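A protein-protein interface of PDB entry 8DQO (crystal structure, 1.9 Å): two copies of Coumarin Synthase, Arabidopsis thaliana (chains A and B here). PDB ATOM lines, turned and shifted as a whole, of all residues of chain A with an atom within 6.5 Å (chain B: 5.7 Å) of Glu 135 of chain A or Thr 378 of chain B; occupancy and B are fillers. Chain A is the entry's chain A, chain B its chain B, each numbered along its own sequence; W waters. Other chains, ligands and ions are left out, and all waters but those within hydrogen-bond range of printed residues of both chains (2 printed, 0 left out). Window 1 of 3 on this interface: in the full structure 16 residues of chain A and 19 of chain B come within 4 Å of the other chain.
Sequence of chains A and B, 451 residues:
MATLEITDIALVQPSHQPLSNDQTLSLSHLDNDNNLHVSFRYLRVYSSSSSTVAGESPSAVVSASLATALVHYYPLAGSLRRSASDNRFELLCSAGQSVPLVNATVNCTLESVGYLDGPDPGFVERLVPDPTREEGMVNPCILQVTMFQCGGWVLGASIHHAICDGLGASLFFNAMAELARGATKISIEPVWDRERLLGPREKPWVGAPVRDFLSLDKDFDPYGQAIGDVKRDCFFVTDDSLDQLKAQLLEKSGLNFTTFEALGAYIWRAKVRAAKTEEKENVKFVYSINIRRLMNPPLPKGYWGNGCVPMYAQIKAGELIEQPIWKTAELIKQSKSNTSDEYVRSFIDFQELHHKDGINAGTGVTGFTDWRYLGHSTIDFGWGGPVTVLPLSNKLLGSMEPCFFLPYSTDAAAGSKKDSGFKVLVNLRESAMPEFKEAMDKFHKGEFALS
Water W2 lies within hydrogen-bond range of NE of Arg 181 of chain B (2.8 Å), OE1 of Glu 134 of chain A (2.9 Å) and SD of Met 137 of chain A (3.2 Å). Water W1 lies within hydrogen-bond range of NE of Arg 181 of chain B (3.3 Å) and SD of Met 137 of chain A (3.7 Å).
The side-chain hydroxyl of Ser 187 of chain B lies within hydrogen-bond range of the guanidinium group of Arg 133 of chain A (3.2 Å). The guanidinium group of Arg 181 of chain B is in hydrogen-bond range of the backbone carbonyl oxygen of Glu 134 of chain A (3.2 Å). OE2 of Glu 135 of chain A lies close to OD1 of Asn 174 of chain B (3.4 Å). ND2 of Asn 139 of chain A sits at hydrogen-bond distance from OG of Ser 377 of chain B, 2.9 Å away.
No position is printed for both chains.
Printed residues of chain A that touch a printed residue of chain B: Thr 132, Arg 133, Glu 134, Glu 135, Val 138 and Asn 139. Hydrophobic or aromatic side chains of chain A that line the printed part of chain B: Val 138. Among the printed residues, no Asp or Glu carboxylate lies within 4 Å of a Lys or Arg side-chain nitrogen of the other chain.
The side-chain carboxylate (OE2) of Glu 134 of chain A lies within salt-bridge range of the guanidinium group (NH1) of Arg 133 of chain A, at 3.2 Å. The side-chain amide oxygen (OD1) of Asn 174 of chain B sits at hydrogen-bond distance from the side-chain hydroxyl (OG1) of Thr 378 of chain B (2.8 Å). OE2 of Glu 178 of chain B is in hydrogen-bond range of OG of Ser 187 of chain B, 2.6 Å away. NH1 of Arg 181 of chain B sits at hydrogen-bond distance from O of Thr 378 of chain B (2.9 Å). NH1 of Arg 181 of chain B lies within hydrogen-bond range of O of Asp 380 of chain B, 3.0 Å away. OG1 of Thr 378 of chain B sits at hydrogen-bond distance from O of Gly 375 of chain B, at 2.9 Å.
Of chain B, only Asn 174 (3.4 Å) and Thr 378 (3.7 Å) come within 4 Å of Glu 135 of chain A. Thr 378 of chain B touches just these residues of chain A: Glu 135 (3.7 Å) and Asn 139 (3.8 Å). Printed residues of chain B within 4 Å of Val 138 of chain A: Arg 181 and Ser 377. Printed residues of chain A within 4 Å of Arg 181 of chain B: Glu 134 and Val 138. Of the printed residues of chain A, Asn 174 of chain B touches Glu 135. Printed residues of chain A within 4 Å of Glu 178 of chain B: Glu 134 (3.1 Å). The nearest residue of chain B that does not touch Glu 135 of chain A is Arg 181 of chain B (4.04 Å). The nearest residue of chain A that does not touch Thr 378 of chain B is Val 138 of chain A (4.3 Å). The nearest printed residue of chain A that does not touch Ser 187 of chain B is Glu 135 of chain A (5.3 Å).
Among the printed residues, pairs that only touch across the chains: Thr 132 of chain A with Ser 187 of chain B (3.7 Å), Glu 134 of chain A with Glu 178 of chain B (3.1 Å), Glu 134 of chain A with Ser 187 of chain B (3.2 Å), Glu 135 of chain A with Thr 378 of chain B (3.7 Å), Val 138 of chain A with Arg 181 of chain B (3.6 Å), Val 138 of chain A with Ser 377 of chain B (3.7 Å) and Asn 139 of chain A with Thr 378 of chain B (3.8 Å).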
ATOM      1  N   SER A  39       6.049 -20.923  -7.301  1.00  0.00           N
ATOM      2  CA  SER A  39       7.308 -20.372  -7.746  1.00  0.00           C
ATOM      3  C   SER A  39       7.503 -20.809  -9.197  1.00  0.00           C
ATOM      4  O   SER A  39       7.212 -21.983  -9.565  1.00  0.00           O
ATOM      5  CB  SER A  39       8.458 -20.824  -6.901  1.00  0.00           C
ATOM      6  OG  SER A  39       8.202 -20.588  -5.513  1.00  0.00           O
ATOM      7  N   ASP A 130      14.346 -24.327  -5.206  1.00  0.00           N
ATOM      8  CA  ASP A 130      13.067 -24.995  -5.461  1.00  0.00           C
ATOM      9  C   ASP A 130      12.169 -24.854  -4.232  1.00  0.00           C
ATOM     10  O   ASP A 130      11.819 -25.837  -3.574  1.00  0.00           O
ATOM     11  CB  ASP A 130      13.274 -26.464  -5.841  1.00  0.00           C
ATOM     12  CG  ASP A 130      12.024 -27.189  -6.305  1.00  0.00           C
ATOM     13  OD1 ASP A 130      11.087 -26.525  -6.793  1.00  0.00           O
ATOM     14  OD2 ASP A 130      11.998 -28.438  -6.172  1.00  0.00           O
ATOM     15  N   PRO A 131      11.779 -23.617  -3.867  1.00  0.00           N
ATOM     16  CA  PRO A 131      10.896 -23.424  -2.715  1.00  0.00           C
ATOM     17  C   PRO A 131       9.475 -23.931  -3.019  1.00  0.00           C
ATOM     18  O   PRO A 131       9.016 -23.901  -4.169  1.00  0.00           O
ATOM     19  CB  PRO A 131      10.947 -21.897  -2.502  1.00  0.00           C
ATOM     20  CG  PRO A 131      11.210 -21.336  -3.888  1.00  0.00           C
ATOM     21  CD  PRO A 131      12.128 -22.353  -4.547  1.00  0.00           C
ATOM     22  N   THR A 132       8.783 -24.400  -1.980  1.00  0.00           N
ATOM     23  CA  THR A 132       7.335 -24.660  -2.058  1.00  0.00           C
ATOM     24  C   THR A 132       6.637 -23.329  -2.360  1.00  0.00           C
ATOM     25  O   THR A 132       7.245 -22.272  -2.251  1.00  0.00           O
ATOM     26  CB  THR A 132       6.771 -25.307  -0.785  1.00  0.00           C
ATOM     27  OG1 THR A 132       6.967 -24.367   0.265  1.00  0.00           O
ATOM     28  CG2 THR A 132       7.411 -26.632  -0.407  1.00  0.00           C
ATOM     29  N   ARG A 133       5.362 -23.399  -2.762  1.00  0.00           N
ATOM     30  CA  ARG A 133       4.532 -22.191  -2.961  1.00  0.00           C
ATOM     31  C   ARG A 133       4.544 -21.328  -1.681  1.00  0.00           C
ATOM     32  O   ARG A 133       4.676 -20.110  -1.758  1.00  0.00           O
ATOM     33  CB  ARG A 133       3.115 -22.584  -3.400  1.00  0.00           C
ATOM     34  CG  ARG A 133       2.377 -23.528  -2.456  1.00  0.00           C
ATOM     35  CD  ARG A 133       0.888 -23.690  -2.753  1.00  0.00           C
ATOM     36  NE  ARG A 133       0.302 -24.970  -2.351  1.00  0.00           N
ATOM     37  CZ  ARG A 133       0.160 -25.452  -1.091  1.00  0.00           C
ATOM     38  NH1 ARG A 133       0.434 -24.743  -0.010  1.00  0.00           N
ATOM     39  NH2 ARG A 133      -0.329 -26.664  -0.916  1.00  0.00           N
ATOM     40  N   GLU A 134       4.469 -21.963  -0.500  1.00  0.00           N
ATOM     41  CA  GLU A 134       4.440 -21.233   0.788  1.00  0.00           C
ATOM     42  C   GLU A 134       5.831 -20.671   1.118  1.00  0.00           C
ATOM     43  O   GLU A 134       5.969 -19.533   1.574  1.00  0.00           O
ATOM     44  CB  GLU A 134       3.847 -22.121   1.879  1.00  0.00           C
ATOM     45  CG  GLU A 134       2.429 -22.593   1.585  1.00  0.00           C
ATOM     46  CD  GLU A 134       1.377 -21.487   1.548  1.00  0.00           C
ATOM     47  OE1 GLU A 134       1.496 -20.520   2.319  1.00  0.00           O
ATOM     48  OE2 GLU A 134       0.426 -21.615   0.751  1.00  0.00           O
ATOM     49  N   GLU A 135       6.885 -21.470   0.901  1.00  0.00           N
ATOM     50  CA  GLU A 135       8.259 -20.999   1.072  1.00  0.00           C
ATOM     51  C   GLU A 135       8.571 -19.822   0.129  1.00  0.00           C
ATOM     52  O   GLU A 135       9.284 -18.919   0.491  1.00  0.00           O
ATOM     53  CB  GLU A 135       9.245 -22.148   0.823  1.00  0.00           C
ATOM     54  CG  GLU A 135       9.385 -23.088   2.006  1.00  0.00           C
ATOM     55  CD  GLU A 135      10.015 -24.444   1.706  1.00  0.00           C
ATOM     56  OE1 GLU A 135      10.289 -24.743   0.532  1.00  0.00           O
ATOM     57  OE2 GLU A 135      10.182 -25.213   2.650  1.00  0.00           O
ATOM     58  N   GLY A 136       8.042 -19.846  -1.089  1.00  0.00           N
ATOM     59  CA  GLY A 136       8.269 -18.801  -2.070  1.00  0.00           C
ATOM     60  C   GLY A 136       7.615 -17.488  -1.676  1.00  0.00           C
ATOM     61  O   GLY A 136       8.007 -16.442  -2.145  1.00  0.00           O
ATOM     62  N   MET A 137       6.622 -17.540  -0.781  1.00  0.00           N
ATOM     63  CA  MET A 137       6.075 -16.311  -0.200  1.00  0.00           C
ATOM     64  C   MET A 137       7.130 -15.575   0.642  1.00  0.00           C
ATOM     65  O   MET A 137       7.211 -14.345   0.605  1.00  0.00           O
ATOM     66  CB  MET A 137       4.828 -16.611   0.639  1.00  0.00           C
ATOM     67  CG  MET A 137       3.650 -17.050  -0.219  1.00  0.00           C
ATOM     68  SD  MET A 137       2.215 -17.442   0.817  1.00  0.00           S
ATOM     69  CE  MET A 137       1.722 -15.774   1.259  1.00  0.00           C
ATOM     70  N   VAL A 138       7.946 -16.312   1.401  1.00  0.00           N
ATOM     71  CA  VAL A 138       8.917 -15.699   2.260  1.00  0.00           C
ATOM     72  C   VAL A 138      10.019 -15.051   1.417  1.00  0.00           C
ATOM     73  O   VAL A 138      10.500 -13.939   1.719  1.00  0.00           O
ATOM     74  CB  VAL A 138       9.525 -16.738   3.222  1.00  0.00           C
ATOM     75  CG1 VAL A 138      10.634 -16.144   4.068  1.00  0.00           C
ATOM     76  CG2 VAL A 138       8.458 -17.382   4.093  1.00  0.00           C
ATOM     77  N   ASN A 139      10.464 -15.802   0.408  1.00  0.00           N
ATOM     78  CA  ASN A 139      11.585 -15.442  -0.462  1.00  0.00           C
ATOM     79  C   ASN A 139      11.112 -15.527  -1.911  1.00  0.00           C
ATOM     80  O   ASN A 139      11.354 -16.502  -2.601  1.00  0.00           O
ATOM     81  CB  ASN A 139      12.790 -16.361  -0.230  1.00  0.00           C
ATOM     82  CG  ASN A 139      13.326 -16.290   1.174  1.00  0.00           C
ATOM     83  OD1 ASN A 139      13.710 -15.216   1.625  1.00  0.00           O
ATOM     84  ND2 ASN A 139      13.407 -17.425   1.848  1.00  0.00           N
ATOM     85  N   PRO A 140      10.303 -14.559  -2.385  1.00  0.00           N
ATOM     86  CA  PRO A 140       9.649 -14.648  -3.691  1.00  0.00           C
ATOM     87  C   PRO A 140      10.487 -14.277  -4.923  1.00  0.00           C
ATOM     88  O   PRO A 140       9.979 -14.291  -6.018  1.00  0.00           O
ATOM     89  CB  PRO A 140       8.485 -13.651  -3.527  1.00  0.00           C
ATOM     90  CG  PRO A 140       9.058 -12.604  -2.619  1.00  0.00           C
ATOM     91  CD  PRO A 140       9.895 -13.373  -1.625  1.00  0.00           C
ATOM     92  N   ILE A 142      14.560 -15.392  -5.827  1.00  0.00           N
ATOM     93  CA  ILE A 142      15.895 -15.901  -5.540  1.00  0.00           C
ATOM     94  C   ILE A 142      16.604 -16.097  -6.874  1.00  0.00           C
ATOM     95  O   ILE A 142      16.041 -16.712  -7.788  1.00  0.00           O
ATOM     96  CB  ILE A 142      15.808 -17.238  -4.789  1.00  0.00           C
ATOM     97  CG1 ILE A 142      14.801 -17.191  -3.634  1.00  0.00           C
ATOM     98  CG2 ILE A 142      17.193 -17.672  -4.350  1.00  0.00           C
ATOM     99  CD1 ILE A 142      14.346 -18.569  -3.165  1.00  0.00           C
ATOM    100  N   HIS A 160       8.120 -16.006  -7.356  1.00  0.00           N
ATOM    101  CA  HIS A 160       6.734 -16.298  -7.064  1.00  0.00           C
ATOM    102  C   HIS A 160       5.870 -15.590  -8.127  1.00  0.00           C
ATOM    103  O   HIS A 160       6.034 -14.383  -8.376  1.00  0.00           O
ATOM    104  CB  HIS A 160       6.367 -15.887  -5.643  1.00  0.00           C
ATOM    105  CG  HIS A 160       5.029 -16.409  -5.244  1.00  0.00           C
ATOM    106  ND1 HIS A 160       3.865 -15.961  -5.830  1.00  0.00           N
ATOM    107  CD2 HIS A 160       4.668 -17.378  -4.379  1.00  0.00           C
ATOM    108  CE1 HIS A 160       2.841 -16.587  -5.279  1.00  0.00           C
ATOM    109  NE2 HIS A 160       3.302 -17.493  -4.438  1.00  0.00           N
ATOM    110  N   ASN B 174       8.478 -26.425   8.723  1.00  0.00           N
ATOM    111  CA  ASN B 174       8.003 -25.629   7.631  1.00  0.00           C
ATOM    112  C   ASN B 174       6.483 -25.752   7.534  1.00  0.00           C
ATOM    113  O   ASN B 174       5.811 -24.775   7.167  1.00  0.00           O
ATOM    114  CB  ASN B 174       8.680 -26.006   6.315  1.00  0.00           C
ATOM    115  CG  ASN B 174       9.874 -25.133   6.027  1.00  0.00           C
ATOM    116  OD1 ASN B 174       9.710 -23.948   5.734  1.00  0.00           O
ATOM    117  ND2 ASN B 174      11.059 -25.709   6.085  1.00  0.00           N
ATOM    118  N   ALA B 177       5.220 -23.453  10.226  1.00  0.00           N
ATOM    119  CA  ALA B 177       5.442 -22.048   9.859  1.00  0.00           C
ATOM    120  C   ALA B 177       4.436 -21.605   8.791  1.00  0.00           C
ATOM    121  O   ALA B 177       3.929 -20.475   8.857  1.00  0.00           O
ATOM    122  CB  ALA B 177       6.858 -21.828   9.381  1.00  0.00           C
ATOM    123  N   GLU B 178       4.185 -22.457   7.785  1.00  0.00           N
ATOM    124  CA  GLU B 178       3.291 -22.047   6.655  1.00  0.00           C
ATOM    125  C   GLU B 178       1.848 -21.950   7.167  1.00  0.00           C
ATOM    126  O   GLU B 178       1.106 -21.041   6.768  1.00  0.00           O
ATOM    127  CB  GLU B 178       3.377 -22.961   5.424  1.00  0.00           C
ATOM    128  CG  GLU B 178       2.849 -24.388   5.623  1.00  0.00           C
ATOM    129  CD  GLU B 178       3.035 -25.316   4.403  1.00  0.00           C
ATOM    130  OE1 GLU B 178       2.866 -26.543   4.576  1.00  0.00           O
ATOM    131  OE2 GLU B 178       3.499 -24.841   3.364  1.00  0.00           O
ATOM    132  N   ARG B 181       1.411 -18.806   8.882  1.00  0.00           N
ATOM    133  CA  ARG B 181       1.362 -17.719   7.870  1.00  0.00           C
ATOM    134  C   ARG B 181       0.022 -17.751   7.118  1.00  0.00           C
ATOM    135  O   ARG B 181      -0.244 -16.903   6.232  1.00  0.00           O
ATOM    136  CB  ARG B 181       2.571 -17.817   6.927  1.00  0.00           C
ATOM    137  CG  ARG B 181       3.904 -17.429   7.558  1.00  0.00           C
ATOM    138  CD  ARG B 181       5.058 -17.325   6.562  1.00  0.00           C
ATOM    139  NE  ARG B 181       5.191 -18.429   5.607  1.00  0.00           N
ATOM    140  CZ  ARG B 181       6.009 -19.461   5.707  1.00  0.00           C
ATOM    141  NH1 ARG B 181       6.755 -19.648   6.796  1.00  0.00           N
ATOM    142  NH2 ARG B 181       6.087 -20.313   4.692  1.00  0.00           N
ATOM    143  N   SER B 187       2.083 -27.667   2.269  1.00  0.00           N
ATOM    144  CA  SER B 187       2.632 -27.747   0.894  1.00  0.00           C
ATOM    145  C   SER B 187       2.964 -29.198   0.494  1.00  0.00           C
ATOM    146  O   SER B 187       2.858 -29.554  -0.677  1.00  0.00           O
ATOM    147  CB  SER B 187       3.850 -26.862   0.757  1.00  0.00           C
ATOM    148  OG  SER B 187       3.470 -25.496   0.800  1.00  0.00           O
ATOM    149  N   GLY B 375      17.200 -24.372   4.533  1.00  0.00           N
ATOM    150  CA  GLY B 375      16.242 -23.294   4.273  1.00  0.00           C
ATOM    151  C   GLY B 375      15.785 -22.642   5.567  1.00  0.00           C
ATOM    152  O   GLY B 375      14.571 -22.548   5.829  1.00  0.00           O
ATOM    153  N   HIS B 376      16.764 -22.180   6.364  1.00  0.00           N
ATOM    154  CA  HIS B 376      16.532 -21.639   7.711  1.00  0.00           C
ATOM    155  C   HIS B 376      15.436 -20.571   7.677  1.00  0.00           C
ATOM    156  O   HIS B 376      14.589 -20.566   8.558  1.00  0.00           O
ATOM    157  CB  HIS B 376      17.819 -21.051   8.311  1.00  0.00           C
ATOM    158  CG  HIS B 376      18.909 -22.057   8.415  1.00  0.00           C
ATOM    159  ND1 HIS B 376      18.840 -23.131   9.279  1.00  0.00           N
ATOM    160  CD2 HIS B 376      20.060 -22.195   7.728  1.00  0.00           C
ATOM    161  CE1 HIS B 376      19.909 -23.887   9.125  1.00  0.00           C
ATOM    162  NE2 HIS B 376      20.673 -23.327   8.186  1.00  0.00           N
ATOM    163  N   SER B 377      15.489 -19.695   6.658  1.00  0.00           N
ATOM    164  CA  SER B 377      14.754 -18.423   6.629  1.00  0.00           C
ATOM    165  C   SER B 377      13.250 -18.644   6.489  1.00  0.00           C
ATOM    166  O   SER B 377      12.498 -17.750   6.809  1.00  0.00           O
ATOM    167  CB  SER B 377      15.247 -17.499   5.538  1.00  0.00           C
ATOM    168  OG  SER B 377      14.949 -18.016   4.251  1.00  0.00           O
ATOM    169  N   THR B 378      12.822 -19.823   6.025  1.00  0.00           N
ATOM    170  CA  THR B 378      11.372 -20.058   5.765  1.00  0.00           C
ATOM    171  C   THR B 378      10.655 -20.497   7.053  1.00  0.00           C
ATOM    172  O   THR B 378       9.431 -20.596   7.085  1.00  0.00           O
ATOM    173  CB  THR B 378      11.179 -21.070   4.634  1.00  0.00           C
ATOM    174  OG1 THR B 378      11.801 -22.303   5.029  1.00  0.00           O
ATOM    175  CG2 THR B 378      11.711 -20.555   3.311  1.00  0.00           C
ATOM    176  N   ILE B 379      11.424 -20.807   8.107  1.00  0.00           N
ATOM    177  CA  ILE B 379      10.819 -21.100   9.410  1.00  0.00           C
ATOM    178  C   ILE B 379      10.471 -19.751  10.047  1.00  0.00           C
ATOM    179  O   ILE B 379      11.094 -19.274  10.997  1.00  0.00           O
ATOM    180  CB  ILE B 379      11.706 -21.997  10.302  1.00  0.00           C
ATOM    181  CG1 ILE B 379      12.280 -23.206   9.553  1.00  0.00           C
ATOM    182  CG2 ILE B 379      10.932 -22.432  11.541  1.00  0.00           C
ATOM    183  CD1 ILE B 379      11.238 -24.128   8.946  1.00  0.00           C
ATOM    184  N   ASP B 380       9.439 -19.134   9.465  1.00  0.00           N
ATOM    185  CA  ASP B 380       8.986 -17.807   9.793  1.00  0.00           C
ATOM    186  C   ASP B 380       7.523 -17.908  10.229  1.00  0.00           C
ATOM    187  O   ASP B 380       6.643 -18.210   9.411  1.00  0.00           O
ATOM    188  CB  ASP B 380       9.121 -16.888   8.581  1.00  0.00           C
ATOM    189  CG  ASP B 380       8.630 -15.472   8.796  1.00  0.00           C
ATOM    190  OD1 ASP B 380       8.108 -15.172   9.899  1.00  0.00           O
ATOM    191  OD2 ASP B 380       8.760 -14.680   7.849  1.00  0.00           O
ATOM    192  N   GLY B 385      12.436 -14.882   9.625  1.00  0.00           N
ATOM    193  CA  GLY B 385      13.288 -16.031   9.780  1.00  0.00           C
ATOM    194  C   GLY B 385      14.169 -15.849  11.014  1.00  0.00           C
ATOM    195  O   GLY B 385      14.261 -14.741  11.545  1.00  0.00           O
ATOM    196  N   PRO B 386      14.776 -16.932  11.542  1.00  0.00           N
ATOM    197  CA  PRO B 386      15.587 -16.836  12.753  1.00  0.00           C
ATOM    198  C   PRO B 386      16.877 -16.037  12.495  1.00  0.00           C
ATOM    199  O   PRO B 386      17.473 -16.174  11.432  1.00  0.00           O
ATOM    200  CB  PRO B 386      15.877 -18.300  13.123  1.00  0.00           C
ATOM    201  CG  PRO B 386      15.738 -19.061  11.832  1.00  0.00           C
ATOM    202  CD  PRO B 386      14.697 -18.306  11.029  1.00  0.00           C
HETATM  203  O   HOH W   1       3.289 -16.134   4.091  1.00  0.00           O
HETATM  204  O   HOH W   2       3.251 -18.635   3.604  1.00  0.00           O
